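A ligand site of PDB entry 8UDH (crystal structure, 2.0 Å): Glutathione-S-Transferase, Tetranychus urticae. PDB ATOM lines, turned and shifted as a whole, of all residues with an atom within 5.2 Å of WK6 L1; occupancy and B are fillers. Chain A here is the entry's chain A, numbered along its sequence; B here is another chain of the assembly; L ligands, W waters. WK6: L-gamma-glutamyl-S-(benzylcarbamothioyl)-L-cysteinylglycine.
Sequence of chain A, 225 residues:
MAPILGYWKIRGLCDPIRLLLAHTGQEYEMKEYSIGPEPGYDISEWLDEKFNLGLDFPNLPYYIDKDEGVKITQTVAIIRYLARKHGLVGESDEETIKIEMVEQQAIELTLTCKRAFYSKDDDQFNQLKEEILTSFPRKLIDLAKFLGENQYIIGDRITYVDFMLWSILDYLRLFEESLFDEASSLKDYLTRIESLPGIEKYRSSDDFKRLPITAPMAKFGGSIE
O4 of WK6 L1 is in salt-bridge range of NZ of Lys 50, 2.6 Å away. The side-chain carboxylate (OE1) of Glu 108 of chain B lies within salt-bridge range of a nitrogen (N4) of WK6 L1 (2.7 Å). A nitrogen (N3) of WK6 L1 sits at hydrogen-bond distance from the side-chain amide oxygen (OD1) of Asn 59 (2.7 Å). A nitrogen (N4) of WK6 L1 lies within hydrogen-bond range of the side-chain amide oxygen (OE1) of Gln 74, 2.8 Å away. NE1 of Trp 8 sits at hydrogen-bond distance from O2 of WK6 L1 (2.8 Å). O of Leu 60 sits at hydrogen-bond distance from N2 of WK6 L1, 2.8 Å away. S1 of WK6 L1 sits close to OH of Tyr 7. O5 of WK6 L1 lies within hydrogen-bond range of N of Thr 75. O5 of WK6 L1 is in hydrogen-bond range of OG1 of Thr 75. O4 of WK6 L1 lies within hydrogen-bond range of NE1 of Trp 46, at 3.1 Å. OH of Tyr 118 sits close to S2 of WK6 L1 (3.4 Å). The side-chain amide nitrogen (ND2) of Asn 59 is in hydrogen-bond range of an oxygen (O6) of WK6 L2 (2.7 Å).
The backbone NH (N) of Leu 13 lies within hydrogen-bond range of the side-chain hydroxyl (OH) of Tyr 7. The backbone NH (N) of Ala 215 sits at hydrogen-bond distance from the side-chain hydroxyl (OH) of Tyr 118, 2.8 Å away. The side-chain hydroxyl (OH) of Tyr 171 sits at hydrogen-bond distance from the backbone carbonyl oxygen (O) of Gly 12 (2.8 Å). N of Gly 12 is in hydrogen-bond range of O of Ile 213, 2.8 Å away.
Residues that only touch WK6 L1: Gly 12, Leu 13, Pro 61, Thr 110, Lys 114, Phe 117, Tyr 171 and Thr 214. 18 residues have an atom within 4 Å of WK6 L1: Tyr 7, Trp 8, Gly 12, Leu 13, Trp 46, Lys 50, Asn 59, Leu 60, Pro 61, Gln 74, Thr 75, Thr 110, Lys 114, Phe 117, Tyr 118, Tyr 171, Thr 214 and Glu 108 of chain B. Along chain A the residues within 4 Å of WK6 L1 span positions 7 to 214. The nearest printed residue that does not touch WK6 L1 is Ile 10 (4.03 Å).
Water W4 lies within hydrogen-bond range of the side-chain amide oxygen of Gln 104 of chain B (2.5 Å), an oxygen (O6) of WK6 L1 (2.7 Å), the backbone NH of Val 76 (3.0 Å) and the backbone NH of Thr 75 (3.2 Å). Water W3 lies within hydrogen-bond range of O of Pro 61 (2.7 Å), N of Gln 74 (2.8 Å) and O5 of WK6 L1 (2.8 Å). Water W2 lies within hydrogen-bond range of the backbone carbonyl oxygen of Gln 104 of chain B and a nitrogen (N4) of WK6 L1.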
ATOM      1  N   TYR A   7     -25.867  13.301  -2.662  1.00  0.00           N
ATOM      2  CA  TYR A   7     -25.354  12.051  -3.186  1.00  0.00           C
ATOM      3  C   TYR A   7     -24.497  11.336  -2.158  1.00  0.00           C
ATOM      4  O   TYR A   7     -24.062  11.899  -1.148  1.00  0.00           O
ATOM      5  CB  TYR A   7     -24.565  12.247  -4.504  1.00  0.00           C
ATOM      6  CG  TYR A   7     -24.402  10.980  -5.328  1.00  0.00           C
ATOM      7  CD1 TYR A   7     -25.513  10.283  -5.793  1.00  0.00           C
ATOM      8  CD2 TYR A   7     -23.152  10.471  -5.647  1.00  0.00           C
ATOM      9  CE1 TYR A   7     -25.381   9.106  -6.522  1.00  0.00           C
ATOM     10  CE2 TYR A   7     -23.008   9.294  -6.383  1.00  0.00           C
ATOM     11  CZ  TYR A   7     -24.129   8.608  -6.811  1.00  0.00           C
ATOM     12  OH  TYR A   7     -23.951   7.458  -7.545  1.00  0.00           O
ATOM     13  N   TRP A   8     -24.256  10.044  -2.447  1.00  0.00           N
ATOM     14  CA  TRP A   8     -23.299   9.246  -1.690  1.00  0.00           C
ATOM     15  C   TRP A   8     -21.927   9.893  -1.794  1.00  0.00           C
ATOM     16  O   TRP A   8     -21.695  10.695  -2.708  1.00  0.00           O
ATOM     17  CB  TRP A   8     -23.273   7.813  -2.237  1.00  0.00           C
ATOM     18  CG  TRP A   8     -24.613   7.141  -2.256  1.00  0.00           C
ATOM     19  CD1 TRP A   8     -25.339   6.779  -3.352  1.00  0.00           C
ATOM     20  CD2 TRP A   8     -25.373   6.721  -1.115  1.00  0.00           C
ATOM     21  NE1 TRP A   8     -26.526   6.201  -2.967  1.00  0.00           N
ATOM     22  CE2 TRP A   8     -26.567   6.132  -1.602  1.00  0.00           C
ATOM     23  CE3 TRP A   8     -25.184   6.813   0.270  1.00  0.00           C
ATOM     24  CZ2 TRP A   8     -27.552   5.643  -0.753  1.00  0.00           C
ATOM     25  CZ3 TRP A   8     -26.154   6.315   1.115  1.00  0.00           C
ATOM     26  CH2 TRP A   8     -27.312   5.725   0.606  1.00  0.00           C
ATOM     27  N   ILE A  10     -19.261   9.043  -3.175  1.00  0.00           N
ATOM     28  CA  ILE A  10     -18.607   8.336  -4.254  1.00  0.00           C
ATOM     29  C   ILE A  10     -18.741   9.215  -5.499  1.00  0.00           C
ATOM     30  O   ILE A  10     -19.573  10.130  -5.510  1.00  0.00           O
ATOM     31  CB  ILE A  10     -19.221   6.935  -4.453  1.00  0.00           C
ATOM     32  CG1 ILE A  10     -20.593   7.019  -5.138  1.00  0.00           C
ATOM     33  CG2 ILE A  10     -19.284   6.162  -3.143  1.00  0.00           C
ATOM     34  CD1 ILE A  10     -21.197   5.681  -5.503  1.00  0.00           C
ATOM     35  N   GLY A  12     -19.571   7.729  -8.700  1.00  0.00           N
ATOM     36  CA  GLY A  12     -20.784   7.077  -9.174  1.00  0.00           C
ATOM     37  C   GLY A  12     -21.462   7.821 -10.332  1.00  0.00           C
ATOM     38  O   GLY A  12     -20.786   8.347 -11.204  1.00  0.00           O
ATOM     39  N   LEU A  13     -22.800   7.877 -10.277  1.00  0.00           N
ATOM     40  CA  LEU A  13     -23.655   8.452 -11.308  1.00  0.00           C
ATOM     41  C   LEU A  13     -23.631   9.978 -11.280  1.00  0.00           C
ATOM     42  O   LEU A  13     -24.057  10.619 -12.229  1.00  0.00           O
ATOM     43  CB  LEU A  13     -25.118   8.040 -11.092  1.00  0.00           C
ATOM     44  CG  LEU A  13     -25.550   6.626 -11.484  1.00  0.00           C
ATOM     45  CD1 LEU A  13     -27.053   6.481 -11.278  1.00  0.00           C
ATOM     46  CD2 LEU A  13     -25.167   6.282 -12.915  1.00  0.00           C
ATOM     47  N   TRP A  46     -29.400   8.727   4.906  1.00  0.00           N
ATOM     48  CA  TRP A  46     -30.243   8.841   3.696  1.00  0.00           C
ATOM     49  C   TRP A  46     -31.617   8.225   3.963  1.00  0.00           C
ATOM     50  O   TRP A  46     -32.614   8.894   3.673  1.00  0.00           O
ATOM     51  CB  TRP A  46     -29.580   8.169   2.491  1.00  0.00           C
ATOM     52  CG  TRP A  46     -30.496   8.026   1.311  1.00  0.00           C
ATOM     53  CD1 TRP A  46     -30.794   6.874   0.646  1.00  0.00           C
ATOM     54  CD2 TRP A  46     -31.240   9.066   0.665  1.00  0.00           C
ATOM     55  NE1 TRP A  46     -31.670   7.130  -0.376  1.00  0.00           N
ATOM     56  CE2 TRP A  46     -31.962   8.465  -0.384  1.00  0.00           C
ATOM     57  CE3 TRP A  46     -31.366  10.443   0.865  1.00  0.00           C
ATOM     58  CZ2 TRP A  46     -32.800   9.201  -1.229  1.00  0.00           C
ATOM     59  CZ3 TRP A  46     -32.195  11.165   0.037  1.00  0.00           C
ATOM     60  CH2 TRP A  46     -32.897  10.552  -0.992  1.00  0.00           C
ATOM     61  N   LYS A  50     -34.896  10.203   2.954  1.00  0.00           N
ATOM     62  CA  LYS A  50     -35.341   9.859   1.610  1.00  0.00           C
ATOM     63  C   LYS A  50     -36.755  10.404   1.344  1.00  0.00           C
ATOM     64  O   LYS A  50     -37.013  11.042   0.303  1.00  0.00           O
ATOM     65  CB  LYS A  50     -35.256   8.339   1.417  1.00  0.00           C
ATOM     66  CG  LYS A  50     -35.912   7.786   0.158  1.00  0.00           C
ATOM     67  CD  LYS A  50     -35.581   6.334  -0.081  1.00  0.00           C
ATOM     68  CE  LYS A  50     -35.971   5.889  -1.468  1.00  0.00           C
ATOM     69  NZ  LYS A  50     -35.372   4.584  -1.844  1.00  0.00           N
ATOM     70  N   PRO A  58     -38.221   9.958  -4.821  1.00  0.00           N
ATOM     71  CA  PRO A  58     -37.105   9.954  -3.866  1.00  0.00           C
ATOM     72  C   PRO A  58     -35.930   9.081  -4.318  1.00  0.00           C
ATOM     73  O   PRO A  58     -36.114   7.916  -4.527  1.00  0.00           O
ATOM     74  CB  PRO A  58     -37.775   9.396  -2.606  1.00  0.00           C
ATOM     75  CG  PRO A  58     -39.193   9.862  -2.722  1.00  0.00           C
ATOM     76  CD  PRO A  58     -39.507   9.659  -4.188  1.00  0.00           C
ATOM     77  N   ASN A  59     -34.754   9.698  -4.449  1.00  0.00           N
ATOM     78  CA  ASN A  59     -33.569   8.960  -4.947  1.00  0.00           C
ATOM     79  C   ASN A  59     -32.301   9.811  -4.837  1.00  0.00           C
ATOM     80  O   ASN A  59     -32.408  11.003  -4.525  1.00  0.00           O
ATOM     81  CB  ASN A  59     -33.741   8.557  -6.413  1.00  0.00           C
ATOM     82  CG  ASN A  59     -33.239   7.161  -6.727  1.00  0.00           C
ATOM     83  OD1 ASN A  59     -32.154   6.779  -6.288  1.00  0.00           O
ATOM     84  ND2 ASN A  59     -34.022   6.396  -7.466  1.00  0.00           N
ATOM     85  N   LEU A  60     -31.160   9.195  -5.070  1.00  0.00           N
ATOM     86  CA  LEU A  60     -29.877   9.936  -5.107  1.00  0.00           C
ATOM     87  C   LEU A  60     -29.266   9.655  -6.492  1.00  0.00           C
ATOM     88  O   LEU A  60     -29.211   8.482  -6.877  1.00  0.00           O
ATOM     89  CB  LEU A  60     -28.966   9.441  -3.986  1.00  0.00           C
ATOM     90  CG  LEU A  60     -29.328   9.882  -2.565  1.00  0.00           C
ATOM     91  CD1 LEU A  60     -28.403   9.247  -1.551  1.00  0.00           C
ATOM     92  CD2 LEU A  60     -29.269  11.399  -2.449  1.00  0.00           C
ATOM     93  N   PRO A  61     -28.849  10.679  -7.244  1.00  0.00           N
ATOM     94  CA  PRO A  61     -28.769  12.046  -6.723  1.00  0.00           C
ATOM     95  C   PRO A  61     -30.037  12.910  -6.704  1.00  0.00           C
ATOM     96  O   PRO A  61     -30.992  12.572  -7.355  1.00  0.00           O
ATOM     97  CB  PRO A  61     -27.790  12.689  -7.714  1.00  0.00           C
ATOM     98  CG  PRO A  61     -28.079  12.001  -9.014  1.00  0.00           C
ATOM     99  CD  PRO A  61     -28.363  10.570  -8.626  1.00  0.00           C
ATOM    100  N   GLN A  74     -33.319  11.972 -10.619  1.00  0.00           N
ATOM    101  CA  GLN A  74     -32.974  11.446 -11.967  1.00  0.00           C
ATOM    102  C   GLN A  74     -31.759  12.210 -12.482  1.00  0.00           C
ATOM    103  O   GLN A  74     -31.900  13.375 -12.852  1.00  0.00           O
ATOM    104  CB  GLN A  74     -34.175  11.414 -12.925  1.00  0.00           C
ATOM    105  CG  GLN A  74     -35.478  10.900 -12.322  1.00  0.00           C
ATOM    106  CD  GLN A  74     -35.360   9.540 -11.688  1.00  0.00           C
ATOM    107  OE1 GLN A  74     -35.017   8.552 -12.335  1.00  0.00           O
ATOM    108  NE2 GLN A  74     -35.676   9.465 -10.400  1.00  0.00           N
ATOM    109  N   THR A  75     -30.606  11.542 -12.525  1.00  0.00           N
ATOM    110  CA  THR A  75     -29.328  12.168 -12.941  1.00  0.00           C
ATOM    111  C   THR A  75     -29.477  12.949 -14.249  1.00  0.00           C
ATOM    112  O   THR A  75     -28.975  14.071 -14.294  1.00  0.00           O
ATOM    113  CB  THR A  75     -28.258  11.078 -13.061  1.00  0.00           C
ATOM    114  OG1 THR A  75     -28.159  10.360 -11.827  1.00  0.00           O
ATOM    115  CG2 THR A  75     -26.895  11.622 -13.440  1.00  0.00           C
ATOM    116  N   VAL A  76     -30.119  12.366 -15.248  1.00  0.00           N
ATOM    117  CA  VAL A  76     -30.237  13.002 -16.593  1.00  0.00           C
ATOM    118  C   VAL A  76     -31.146  14.237 -16.501  1.00  0.00           C
ATOM    119  O   VAL A  76     -30.799  15.245 -17.107  1.00  0.00           O
ATOM    120  CB  VAL A  76     -30.712  11.997 -17.662  1.00  0.00           C
ATOM    121  CG1 VAL A  76     -30.882  12.650 -19.027  1.00  0.00           C
ATOM    122  CG2 VAL A  76     -29.789  10.795 -17.760  1.00  0.00           C
ATOM    123  N   THR A 110     -22.142   3.518 -19.450  1.00  0.00           N
ATOM    124  CA  THR A 110     -22.126   3.729 -17.975  1.00  0.00           C
ATOM    125  C   THR A 110     -22.943   2.630 -17.283  1.00  0.00           C
ATOM    126  O   THR A 110     -22.466   2.095 -16.296  1.00  0.00           O
ATOM    127  CB  THR A 110     -22.570   5.157 -17.622  1.00  0.00           C
ATOM    128  OG1 THR A 110     -21.811   6.083 -18.389  1.00  0.00           O
ATOM    129  CG2 THR A 110     -22.438   5.460 -16.150  1.00  0.00           C
ATOM    130  N   CYS A 113     -21.145  -0.703 -17.360  1.00  0.00           N
ATOM    131  CA  CYS A 113     -20.113  -0.695 -16.324  1.00  0.00           C
ATOM    132  C   CYS A 113     -20.704  -0.838 -14.911  1.00  0.00           C
ATOM    133  O   CYS A 113     -20.171  -1.609 -14.121  1.00  0.00           O
ATOM    134  CB  CYS A 113     -19.238   0.544 -16.424  1.00  0.00           C
ATOM    135  SG  CYS A 113     -18.218   0.454 -17.918  1.00  0.00           S
ATOM    136  N   LYS A 114     -21.779  -0.100 -14.629  1.00  0.00           N
ATOM    137  CA  LYS A 114     -22.460  -0.140 -13.346  1.00  0.00           C
ATOM    138  C   LYS A 114     -22.876  -1.573 -13.028  1.00  0.00           C
ATOM    139  O   LYS A 114     -22.624  -2.064 -11.923  1.00  0.00           O
ATOM    140  CB  LYS A 114     -23.670   0.800 -13.386  1.00  0.00           C
ATOM    141  CG  LYS A 114     -24.449   0.931 -12.082  1.00  0.00           C
ATOM    142  CD  LYS A 114     -25.734   1.724 -12.242  1.00  0.00           C
ATOM    143  CE  LYS A 114     -26.180   2.456 -10.992  1.00  0.00           C
ATOM    144  NZ  LYS A 114     -26.061   1.620  -9.773  1.00  0.00           N
ATOM    145  N   PHE A 117     -19.761  -3.570 -12.254  1.00  0.00           N
ATOM    146  CA  PHE A 117     -19.108  -3.164 -11.019  1.00  0.00           C
ATOM    147  C   PHE A 117     -19.861  -3.693  -9.791  1.00  0.00           C
ATOM    148  O   PHE A 117     -19.226  -4.018  -8.796  1.00  0.00           O
ATOM    149  CB  PHE A 117     -18.917  -1.641 -10.985  1.00  0.00           C
ATOM    150  CG  PHE A 117     -17.949  -1.052 -12.007  1.00  0.00           C
ATOM    151  CD1 PHE A 117     -17.183  -1.859 -12.864  1.00  0.00           C
ATOM    152  CD2 PHE A 117     -17.821   0.326 -12.155  1.00  0.00           C
ATOM    153  CE1 PHE A 117     -16.330  -1.298 -13.814  1.00  0.00           C
ATOM    154  CE2 PHE A 117     -16.966   0.878 -13.102  1.00  0.00           C
ATOM    155  CZ  PHE A 117     -16.219   0.070 -13.921  1.00  0.00           C
ATOM    156  N   TYR A 118     -21.189  -3.820  -9.876  1.00  0.00           N
ATOM    157  CA  TYR A 118     -22.033  -4.227  -8.751  1.00  0.00           C
ATOM    158  C   TYR A 118     -22.561  -5.644  -8.944  1.00  0.00           C
ATOM    159  O   TYR A 118     -23.592  -5.987  -8.376  1.00  0.00           O
ATOM    160  CB  TYR A 118     -23.204  -3.251  -8.574  1.00  0.00           C
ATOM    161  CG  TYR A 118     -22.788  -1.900  -8.040  1.00  0.00           C
ATOM    162  CD1 TYR A 118     -22.520  -1.701  -6.694  1.00  0.00           C
ATOM    163  CD2 TYR A 118     -22.610  -0.831  -8.895  1.00  0.00           C
ATOM    164  CE1 TYR A 118     -22.128  -0.466  -6.209  1.00  0.00           C
ATOM    165  CE2 TYR A 118     -22.215   0.408  -8.431  1.00  0.00           C
ATOM    166  CZ  TYR A 118     -21.957   0.605  -7.088  1.00  0.00           C
ATOM    167  OH  TYR A 118     -21.575   1.854  -6.621  1.00  0.00           O
ATOM    168  N   TYR A 171     -13.537   6.354 -16.030  1.00  0.00           N
ATOM    169  CA  TYR A 171     -13.769   5.078 -15.326  1.00  0.00           C
ATOM    170  C   TYR A 171     -13.156   3.933 -16.132  1.00  0.00           C
ATOM    171  O   TYR A 171     -12.500   3.087 -15.533  1.00  0.00           O
ATOM    172  CB  TYR A 171     -15.268   4.843 -15.138  1.00  0.00           C
ATOM    173  CG  TYR A 171     -15.988   5.780 -14.196  1.00  0.00           C
ATOM    174  CD1 TYR A 171     -15.314   6.708 -13.426  1.00  0.00           C
ATOM    175  CD2 TYR A 171     -17.366   5.723 -14.077  1.00  0.00           C
ATOM    176  CE1 TYR A 171     -15.987   7.563 -12.566  1.00  0.00           C
ATOM    177  CE2 TYR A 171     -18.056   6.564 -13.219  1.00  0.00           C
ATOM    178  CZ  TYR A 171     -17.367   7.489 -12.465  1.00  0.00           C
ATOM    179  OH  TYR A 171     -18.051   8.315 -11.621  1.00  0.00           O
ATOM    180  N   ILE A 213     -14.808   5.450  -6.849  1.00  0.00           N
ATOM    181  CA  ILE A 213     -15.710   5.437  -7.996  1.00  0.00           C
ATOM    182  C   ILE A 213     -17.077   4.881  -7.583  1.00  0.00           C
ATOM    183  O   ILE A 213     -18.116   5.475  -7.885  1.00  0.00           O
ATOM    184  CB  ILE A 213     -15.091   4.660  -9.174  1.00  0.00           C
ATOM    185  CG1 ILE A 213     -13.790   5.317  -9.635  1.00  0.00           C
ATOM    186  CG2 ILE A 213     -16.105   4.477 -10.295  1.00  0.00           C
ATOM    187  CD1 ILE A 213     -12.979   4.501 -10.639  1.00  0.00           C
ATOM    188  N   THR A 214     -17.040   3.736  -6.904  1.00  0.00           N
ATOM    189  CA  THR A 214     -18.295   3.028  -6.556  1.00  0.00           C
ATOM    190  C   THR A 214     -18.455   2.847  -5.052  1.00  0.00           C
ATOM    191  O   THR A 214     -17.515   3.168  -4.315  1.00  0.00           O
ATOM    192  CB  THR A 214     -18.305   1.652  -7.237  1.00  0.00           C
ATOM    193  OG1 THR A 214     -17.208   0.909  -6.703  1.00  0.00           O
ATOM    194  CG2 THR A 214     -18.201   1.716  -8.744  1.00  0.00           C
ATOM    195  N   ALA A 215     -19.602   2.330  -4.630  1.00  0.00           N
ATOM    196  CA  ALA A 215     -19.895   2.104  -3.195  1.00  0.00           C
ATOM    197  C   ALA A 215     -19.082   0.921  -2.661  1.00  0.00           C
ATOM    198  O   ALA A 215     -18.629   0.109  -3.477  1.00  0.00           O
ATOM    199  CB  ALA A 215     -21.373   1.916  -3.003  1.00  0.00           C
ATOM    200  N   GLN B 104     -37.040   9.457 -17.262  1.00  0.00           N
ATOM    201  CA  GLN B 104     -35.994   8.640 -16.604  1.00  0.00           C
ATOM    202  C   GLN B 104     -36.615   7.532 -15.746  1.00  0.00           C
ATOM    203  O   GLN B 104     -36.110   6.426 -15.764  1.00  0.00           O
ATOM    204  CB  GLN B 104     -35.087   9.597 -15.829  1.00  0.00           C
ATOM    205  CG  GLN B 104     -34.361  10.577 -16.739  1.00  0.00           C
ATOM    206  CD  GLN B 104     -33.446   9.824 -17.667  1.00  0.00           C
ATOM    207  OE1 GLN B 104     -32.588   9.074 -17.232  1.00  0.00           O
ATOM    208  NE2 GLN B 104     -33.636  10.014 -18.971  1.00  0.00           N
ATOM    209  N   GLU B 108     -36.030   3.551 -16.352  1.00  0.00           N
ATOM    210  CA  GLU B 108     -35.503   2.726 -15.235  1.00  0.00           C
ATOM    211  C   GLU B 108     -36.365   1.454 -15.111  1.00  0.00           C
ATOM    212  O   GLU B 108     -35.807   0.370 -15.056  1.00  0.00           O
ATOM    213  CB  GLU B 108     -35.462   3.572 -13.976  1.00  0.00           C
ATOM    214  CG  GLU B 108     -35.308   2.786 -12.686  1.00  0.00           C
ATOM    215  CD  GLU B 108     -35.507   3.625 -11.428  1.00  0.00           C
ATOM    216  OE1 GLU B 108     -34.701   4.536 -11.197  1.00  0.00           O
ATOM    217  OE2 GLU B 108     -36.476   3.365 -10.704  1.00  0.00           O
HETATM  218  S1  WK6 L   1     -26.197   5.498  -7.891  1.00  0.00           S
HETATM  219  C1  WK6 L   1     -20.633   3.762 -12.882  1.00  0.00           C
HETATM  220  C2  WK6 L   1     -19.985   3.338 -11.737  1.00  0.00           C
HETATM  221  C3  WK6 L   1     -20.606   3.383 -10.483  1.00  0.00           C
HETATM  222  C4  WK6 L   1     -21.878   3.870 -10.283  1.00  0.00           C
HETATM  223  C5  WK6 L   1     -22.509   4.317 -11.430  1.00  0.00           C
HETATM  224  C6  WK6 L   1     -21.897   4.277 -12.698  1.00  0.00           C
HETATM  225  C7  WK6 L   1     -22.460   3.876  -8.877  1.00  0.00           C
HETATM  226  N1  WK6 L   1     -23.770   4.539  -8.738  1.00  0.00           N
HETATM  227  C8  WK6 L   1     -24.752   4.525  -7.742  1.00  0.00           C
HETATM  228  S2  WK6 L   1     -24.517   3.569  -6.490  1.00  0.00           S
HETATM  229  C9  WK6 L   1     -31.373   6.065 -10.432  1.00  0.00           C
HETATM  230  C10 WK6 L   1     -30.637   6.511  -9.184  1.00  0.00           C
HETATM  231  C11 WK6 L   1     -29.910   5.346  -8.519  1.00  0.00           C
HETATM  232  O1  WK6 L   1     -29.849   4.211  -9.021  1.00  0.00           O
HETATM  233  N2  WK6 L   1     -29.324   5.721  -7.380  1.00  0.00           N
HETATM  234  C12 WK6 L   1     -28.541   4.865  -6.484  1.00  0.00           C
HETATM  235  C13 WK6 L   1     -27.136   5.507  -6.394  1.00  0.00           C
HETATM  236  C14 WK6 L   1     -29.116   4.898  -5.094  1.00  0.00           C
HETATM  237  O2  WK6 L   1     -28.464   4.557  -4.155  1.00  0.00           O
HETATM  238  N3  WK6 L   1     -30.352   5.354  -4.876  1.00  0.00           N
HETATM  239  C15 WK6 L   1     -30.947   5.489  -3.553  1.00  0.00           C
HETATM  240  C16 WK6 L   1     -32.179   4.670  -3.329  1.00  0.00           C
HETATM  241  O3  WK6 L   1     -32.458   3.751  -4.140  1.00  0.00           O
HETATM  242  O4  WK6 L   1     -32.855   5.014  -2.336  1.00  0.00           O
HETATM  243  C17 WK6 L   1     -32.262   7.153 -11.090  1.00  0.00           C
HETATM  244  C18 WK6 L   1     -31.279   8.164 -11.677  1.00  0.00           C
HETATM  245  O5  WK6 L   1     -30.693   8.996 -10.926  1.00  0.00           O
HETATM  246  O6  WK6 L   1     -31.049   8.063 -12.908  1.00  0.00           O
HETATM  247  N4  WK6 L   1     -33.136   6.513 -12.117  1.00  0.00           N
HETATM  248  S1  WK6 L   2     -31.505   2.460 -14.979  1.00  0.00           S
HETATM  249  C1  WK6 L   2     -26.189   7.268 -16.502  1.00  0.00           C
HETATM  250  C2  WK6 L   2     -27.081   8.159 -15.974  1.00  0.00           C
HETATM  251  C3  WK6 L   2     -28.188   7.707 -15.278  1.00  0.00           C
HETATM  252  C4  WK6 L   2     -28.408   6.349 -15.119  1.00  0.00           C
HETATM  253  C5  WK6 L   2     -27.494   5.460 -15.652  1.00  0.00           C
HETATM  254  C6  WK6 L   2     -26.392   5.924 -16.342  1.00  0.00           C
HETATM  255  C7  WK6 L   2     -29.614   5.851 -14.352  1.00  0.00           C
HETATM  256  N1  WK6 L   2     -30.205   4.666 -14.941  1.00  0.00           N
HETATM  257  C8  WK6 L   2     -30.318   3.522 -14.251  1.00  0.00           C
HETATM  258  S2  WK6 L   2     -29.436   3.154 -12.893  1.00  0.00           S
HETATM  259  C9  WK6 L   2     -32.353   2.336  -9.529  1.00  0.00           C
HETATM  260  C10 WK6 L   2     -32.975   1.092 -10.152  1.00  0.00           C
HETATM  261  C11 WK6 L   2     -32.183   0.649 -11.375  1.00  0.00           C
HETATM  262  O1  WK6 L   2     -31.003   0.335 -11.294  1.00  0.00           O
HETATM  263  N2  WK6 L   2     -32.870   0.617 -12.521  1.00  0.00           N
HETATM  264  C12 WK6 L   2     -32.356   0.102 -13.791  1.00  0.00           C
HETATM  265  C13 WK6 L   2     -31.118   0.855 -14.254  1.00  0.00           C
HETATM  266  C14 WK6 L   2     -32.080  -1.405 -13.815  1.00  0.00           C
HETATM  267  O2  WK6 L   2     -31.883  -1.953 -14.897  1.00  0.00           O
HETATM  268  N3  WK6 L   2     -32.050  -2.039 -12.647  1.00  0.00           N
HETATM  269  C15 WK6 L   2     -32.001  -3.486 -12.569  1.00  0.00           C
HETATM  270  C16 WK6 L   2     -30.693  -4.078 -13.106  1.00  0.00           C
HETATM  271  O3  WK6 L   2     -29.818  -3.277 -13.503  1.00  0.00           O
HETATM  272  O4  WK6 L   2     -30.600  -5.313 -13.118  1.00  0.00           O
HETATM  273  C17 WK6 L   2     -32.376   2.346  -7.997  1.00  0.00           C
HETATM  274  C18 WK6 L   2     -33.779   2.626  -7.453  1.00  0.00           C
HETATM  275  O5  WK6 L   2     -34.278   1.761  -6.694  1.00  0.00           O
HETATM  276  O6  WK6 L   2     -34.314   3.696  -7.789  1.00  0.00           O
HETATM  277  N4  WK6 L   2     -31.891   1.043  -7.470  1.00  0.00           N
HETATM  278  O   HOH W   1     -25.045   1.917  -4.223  1.00  0.00           O
HETATM  279  O   HOH W   2     -33.320   6.208 -15.413  1.00  0.00           O
HETATM  280  O   HOH W   3     -31.811  10.477  -8.850  1.00  0.00           O
HETATM  281  O   HOH W   4     -31.542   9.709 -15.011  1.00  0.00           O
